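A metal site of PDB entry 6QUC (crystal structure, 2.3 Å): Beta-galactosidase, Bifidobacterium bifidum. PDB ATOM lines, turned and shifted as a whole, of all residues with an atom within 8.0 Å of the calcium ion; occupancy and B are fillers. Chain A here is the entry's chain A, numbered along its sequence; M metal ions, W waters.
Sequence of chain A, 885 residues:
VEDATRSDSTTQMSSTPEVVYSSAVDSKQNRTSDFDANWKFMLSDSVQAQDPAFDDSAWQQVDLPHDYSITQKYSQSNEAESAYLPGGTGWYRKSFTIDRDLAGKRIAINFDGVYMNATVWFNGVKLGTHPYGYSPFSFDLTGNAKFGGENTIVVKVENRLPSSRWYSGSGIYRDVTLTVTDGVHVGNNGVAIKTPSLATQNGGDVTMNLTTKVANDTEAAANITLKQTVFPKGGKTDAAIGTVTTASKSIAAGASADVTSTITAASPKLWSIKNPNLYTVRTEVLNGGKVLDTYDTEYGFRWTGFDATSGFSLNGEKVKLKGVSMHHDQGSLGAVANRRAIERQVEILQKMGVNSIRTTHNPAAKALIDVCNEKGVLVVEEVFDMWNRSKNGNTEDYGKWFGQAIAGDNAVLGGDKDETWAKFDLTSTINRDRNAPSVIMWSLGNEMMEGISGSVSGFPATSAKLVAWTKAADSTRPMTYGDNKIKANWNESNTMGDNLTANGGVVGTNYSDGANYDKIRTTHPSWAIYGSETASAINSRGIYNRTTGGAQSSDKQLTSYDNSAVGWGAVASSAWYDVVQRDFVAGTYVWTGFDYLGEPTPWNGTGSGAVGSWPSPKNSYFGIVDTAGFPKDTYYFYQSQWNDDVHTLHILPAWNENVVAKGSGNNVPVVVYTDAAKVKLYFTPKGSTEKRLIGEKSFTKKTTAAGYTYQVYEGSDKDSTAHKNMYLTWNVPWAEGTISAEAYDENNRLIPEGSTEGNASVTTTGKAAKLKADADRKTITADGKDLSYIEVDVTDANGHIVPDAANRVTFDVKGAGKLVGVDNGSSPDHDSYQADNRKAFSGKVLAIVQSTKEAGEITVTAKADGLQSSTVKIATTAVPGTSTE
A ring nitrogen (ND1) of His 647 sits close to the side-chain carboxylate (OD2) of Asp 675. OD1 of Asp 675 lies within hydrogen-bond range of N of Thr 648 (2.8 Å). The side-chain amide oxygen (OD1) of Asn 643 lies within hydrogen-bond range of the backbone NH (N) of Asp 645 (3.0 Å).
The nearest printed residue that does not touch the calcium ion is Asp 644 (4.1 Å).
The calcium ion is bound by the backbone carbonyl oxygen of Val 646, water W1, the side-chain carboxylate of Asp 675, the backbone carbonyl oxygen of Asn 643 and water W2. The calcium ion has five donor atoms within binding distance.
Water W2 lies within hydrogen-bond range of the side-chain hydroxyl (OG1) of Thr 648 and the backbone carbonyl oxygen (O) of Gln 639.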
ATOM      1  N   TYR A 638     -22.732 -26.524  -0.993  1.00  0.00           N
ATOM      2  CA  TYR A 638     -22.004 -26.863   0.228  1.00  0.00           C
ATOM      3  C   TYR A 638     -20.792 -25.972   0.406  1.00  0.00           C
ATOM      4  O   TYR A 638     -20.539 -25.477   1.510  1.00  0.00           O
ATOM      5  CB  TYR A 638     -21.601 -28.335   0.195  1.00  0.00           C
ATOM      6  CG  TYR A 638     -22.716 -29.290   0.548  1.00  0.00           C
ATOM      7  CD1 TYR A 638     -23.138 -29.429   1.869  1.00  0.00           C
ATOM      8  CD2 TYR A 638     -23.350 -30.048  -0.425  1.00  0.00           C
ATOM      9  CE1 TYR A 638     -24.160 -30.298   2.204  1.00  0.00           C
ATOM     10  CE2 TYR A 638     -24.363 -30.926  -0.095  1.00  0.00           C
ATOM     11  CZ  TYR A 638     -24.763 -31.046   1.230  1.00  0.00           C
ATOM     12  OH  TYR A 638     -25.785 -31.915   1.565  1.00  0.00           O
ATOM     13  N   GLN A 639     -20.027 -25.745  -0.674  1.00  0.00           N
ATOM     14  CA  GLN A 639     -18.845 -24.888  -0.569  1.00  0.00           C
ATOM     15  C   GLN A 639     -19.225 -23.482  -0.123  1.00  0.00           C
ATOM     16  O   GLN A 639     -18.487 -22.855   0.649  1.00  0.00           O
ATOM     17  CB  GLN A 639     -18.111 -24.839  -1.907  1.00  0.00           C
ATOM     18  CG  GLN A 639     -16.758 -24.143  -1.799  1.00  0.00           C
ATOM     19  CD  GLN A 639     -16.111 -23.914  -3.142  1.00  0.00           C
ATOM     20  OE1 GLN A 639     -16.530 -23.023  -3.893  1.00  0.00           O
ATOM     21  NE2 GLN A 639     -15.096 -24.708  -3.467  1.00  0.00           N
ATOM     22  N   SER A 640     -20.359 -22.968  -0.607  1.00  0.00           N
ATOM     23  CA  SER A 640     -20.809 -21.642  -0.174  1.00  0.00           C
ATOM     24  C   SER A 640     -21.170 -21.638   1.305  1.00  0.00           C
ATOM     25  O   SER A 640     -21.090 -20.593   1.949  1.00  0.00           O
ATOM     26  CB  SER A 640     -22.003 -21.178  -1.017  1.00  0.00           C
ATOM     27  OG  SER A 640     -23.194 -21.872  -0.688  1.00  0.00           O
ATOM     28  N   GLN A 641     -21.551 -22.788   1.852  1.00  0.00           N
ATOM     29  CA  GLN A 641     -21.961 -22.883   3.250  1.00  0.00           C
ATOM     30  C   GLN A 641     -20.811 -23.180   4.194  1.00  0.00           C
ATOM     31  O   GLN A 641     -20.880 -22.808   5.370  1.00  0.00           O
ATOM     32  CB  GLN A 641     -23.033 -23.975   3.403  1.00  0.00           C
ATOM     33  CG  GLN A 641     -24.247 -23.764   2.528  1.00  0.00           C
ATOM     34  CD  GLN A 641     -24.934 -22.461   2.810  1.00  0.00           C
ATOM     35  OE1 GLN A 641     -25.411 -22.232   3.917  1.00  0.00           O
ATOM     36  NE2 GLN A 641     -24.980 -21.580   1.815  1.00  0.00           N
ATOM     37  N   TRP A 642     -19.761 -23.835   3.722  1.00  0.00           N
ATOM     38  CA  TRP A 642     -18.802 -24.462   4.613  1.00  0.00           C
ATOM     39  C   TRP A 642     -17.386 -23.906   4.522  1.00  0.00           C
ATOM     40  O   TRP A 642     -16.687 -23.908   5.535  1.00  0.00           O
ATOM     41  CB  TRP A 642     -18.735 -25.971   4.336  1.00  0.00           C
ATOM     42  CG  TRP A 642     -19.977 -26.710   4.761  1.00  0.00           C
ATOM     43  CD1 TRP A 642     -21.071 -26.192   5.378  1.00  0.00           C
ATOM     44  CD2 TRP A 642     -20.227 -28.119   4.615  1.00  0.00           C
ATOM     45  NE1 TRP A 642     -22.003 -27.183   5.612  1.00  0.00           N
ATOM     46  CE2 TRP A 642     -21.504 -28.367   5.155  1.00  0.00           C
ATOM     47  CE3 TRP A 642     -19.497 -29.185   4.071  1.00  0.00           C
ATOM     48  CZ2 TRP A 642     -22.068 -29.646   5.170  1.00  0.00           C
ATOM     49  CZ3 TRP A 642     -20.070 -30.446   4.096  1.00  0.00           C
ATOM     50  CH2 TRP A 642     -21.334 -30.674   4.638  1.00  0.00           C
ATOM     51  N   ASN A 643     -16.952 -23.449   3.355  1.00  0.00           N
ATOM     52  CA  ASN A 643     -15.555 -23.098   3.121  1.00  0.00           C
ATOM     53  C   ASN A 643     -15.388 -21.594   3.352  1.00  0.00           C
ATOM     54  O   ASN A 643     -15.731 -20.782   2.490  1.00  0.00           O
ATOM     55  CB  ASN A 643     -15.128 -23.512   1.714  1.00  0.00           C
ATOM     56  CG  ASN A 643     -13.635 -23.429   1.513  1.00  0.00           C
ATOM     57  OD1 ASN A 643     -12.930 -22.691   2.209  1.00  0.00           O
ATOM     58  ND2 ASN A 643     -13.121 -24.195   0.549  1.00  0.00           N
ATOM     59  N   ASP A 644     -14.843 -21.235   4.514  1.00  0.00           N
ATOM     60  CA  ASP A 644     -14.647 -19.849   4.889  1.00  0.00           C
ATOM     61  C   ASP A 644     -13.355 -19.251   4.322  1.00  0.00           C
ATOM     62  O   ASP A 644     -13.106 -18.059   4.545  1.00  0.00           O
ATOM     63  CB  ASP A 644     -14.660 -19.706   6.415  1.00  0.00           C
ATOM     64  CG  ASP A 644     -16.005 -20.071   7.015  1.00  0.00           C
ATOM     65  OD1 ASP A 644     -17.045 -19.844   6.350  1.00  0.00           O
ATOM     66  OD2 ASP A 644     -16.033 -20.596   8.154  1.00  0.00           O
ATOM     67  N   ASP A 645     -12.535 -20.046   3.639  1.00  0.00           N
ATOM     68  CA  ASP A 645     -11.305 -19.550   3.036  1.00  0.00           C
ATOM     69  C   ASP A 645     -11.445 -19.292   1.540  1.00  0.00           C
ATOM     70  O   ASP A 645     -10.430 -19.092   0.855  1.00  0.00           O
ATOM     71  CB  ASP A 645     -10.160 -20.547   3.288  1.00  0.00           C
ATOM     72  CG  ASP A 645      -9.940 -20.821   4.759  1.00  0.00           C
ATOM     73  OD1 ASP A 645     -10.243 -19.945   5.594  1.00  0.00           O
ATOM     74  OD2 ASP A 645      -9.459 -21.929   5.097  1.00  0.00           O
ATOM     75  N   VAL A 646     -12.661 -19.289   1.010  1.00  0.00           N
ATOM     76  CA  VAL A 646     -12.888 -19.218  -0.424  1.00  0.00           C
ATOM     77  C   VAL A 646     -14.209 -18.503  -0.674  1.00  0.00           C
ATOM     78  O   VAL A 646     -15.095 -18.493   0.184  1.00  0.00           O
ATOM     79  CB  VAL A 646     -12.852 -20.630  -1.071  1.00  0.00           C
ATOM     80  CG1 VAL A 646     -14.251 -21.083  -1.495  1.00  0.00           C
ATOM     81  CG2 VAL A 646     -11.875 -20.666  -2.218  1.00  0.00           C
ATOM     82  N   HIS A 647     -14.329 -17.884  -1.844  1.00  0.00           N
ATOM     83  CA  HIS A 647     -15.575 -17.277  -2.271  1.00  0.00           C
ATOM     84  C   HIS A 647     -16.158 -18.090  -3.427  1.00  0.00           C
ATOM     85  O   HIS A 647     -15.437 -18.478  -4.341  1.00  0.00           O
ATOM     86  CB  HIS A 647     -15.364 -15.822  -2.695  1.00  0.00           C
ATOM     87  CG  HIS A 647     -15.149 -14.887  -1.545  1.00  0.00           C
ATOM     88  ND1 HIS A 647     -15.727 -15.090  -0.307  1.00  0.00           N
ATOM     89  CD2 HIS A 647     -14.417 -13.750  -1.439  1.00  0.00           C
ATOM     90  CE1 HIS A 647     -15.361 -14.120   0.504  1.00  0.00           C
ATOM     91  NE2 HIS A 647     -14.572 -13.298  -0.151  1.00  0.00           N
ATOM     92  N   THR A 648     -17.455 -18.350  -3.349  1.00  0.00           N
ATOM     93  CA  THR A 648     -18.147 -19.232  -4.288  1.00  0.00           C
ATOM     94  C   THR A 648     -19.148 -18.423  -5.104  1.00  0.00           C
ATOM     95  O   THR A 648     -19.864 -17.578  -4.567  1.00  0.00           O
ATOM     96  CB  THR A 648     -18.867 -20.360  -3.555  1.00  0.00           C
ATOM     97  OG1 THR A 648     -17.945 -21.067  -2.720  1.00  0.00           O
ATOM     98  CG2 THR A 648     -19.486 -21.330  -4.553  1.00  0.00           C
ATOM     99  N   THR A 674     -23.807 -19.206  -3.769  1.00  0.00           N
ATOM    100  CA  THR A 674     -22.782 -18.230  -3.454  1.00  0.00           C
ATOM    101  C   THR A 674     -22.766 -17.947  -1.966  1.00  0.00           C
ATOM    102  O   THR A 674     -23.779 -18.130  -1.270  1.00  0.00           O
ATOM    103  CB  THR A 674     -22.986 -16.931  -4.242  1.00  0.00           C
ATOM    104  OG1 THR A 674     -21.899 -16.036  -3.958  1.00  0.00           O
ATOM    105  CG2 THR A 674     -24.295 -16.269  -3.835  1.00  0.00           C
ATOM    106  N   ASP A 675     -21.612 -17.498  -1.480  1.00  0.00           N
ATOM    107  CA  ASP A 675     -21.472 -16.998  -0.125  1.00  0.00           C
ATOM    108  C   ASP A 675     -21.445 -15.471  -0.075  1.00  0.00           C
ATOM    109  O   ASP A 675     -21.303 -14.901   1.003  1.00  0.00           O
ATOM    110  CB  ASP A 675     -20.198 -17.545   0.522  1.00  0.00           C
ATOM    111  CG  ASP A 675     -18.941 -17.116  -0.203  1.00  0.00           C
ATOM    112  OD1 ASP A 675     -18.984 -16.953  -1.437  1.00  0.00           O
ATOM    113  OD2 ASP A 675     -17.901 -16.938   0.479  1.00  0.00           O
ATOM    114  N   ALA A 676     -21.582 -14.816  -1.225  1.00  0.00           N
ATOM    115  CA  ALA A 676     -21.569 -13.359  -1.269  1.00  0.00           C
ATOM    116  C   ALA A 676     -22.831 -12.796  -0.621  1.00  0.00           C
ATOM    117  O   ALA A 676     -23.843 -13.482  -0.443  1.00  0.00           O
ATOM    118  CB  ALA A 676     -21.460 -12.857  -2.698  1.00  0.00           C
HETATM  119 CA    CA M   1     -16.802 -18.788   1.603  1.00  0.00          CA
HETATM  120  O   HOH W   1     -18.751 -19.720   2.601  1.00  0.00           O
HETATM  121  O   HOH W   2     -17.878 -20.161  -0.204  1.00  0.00           O
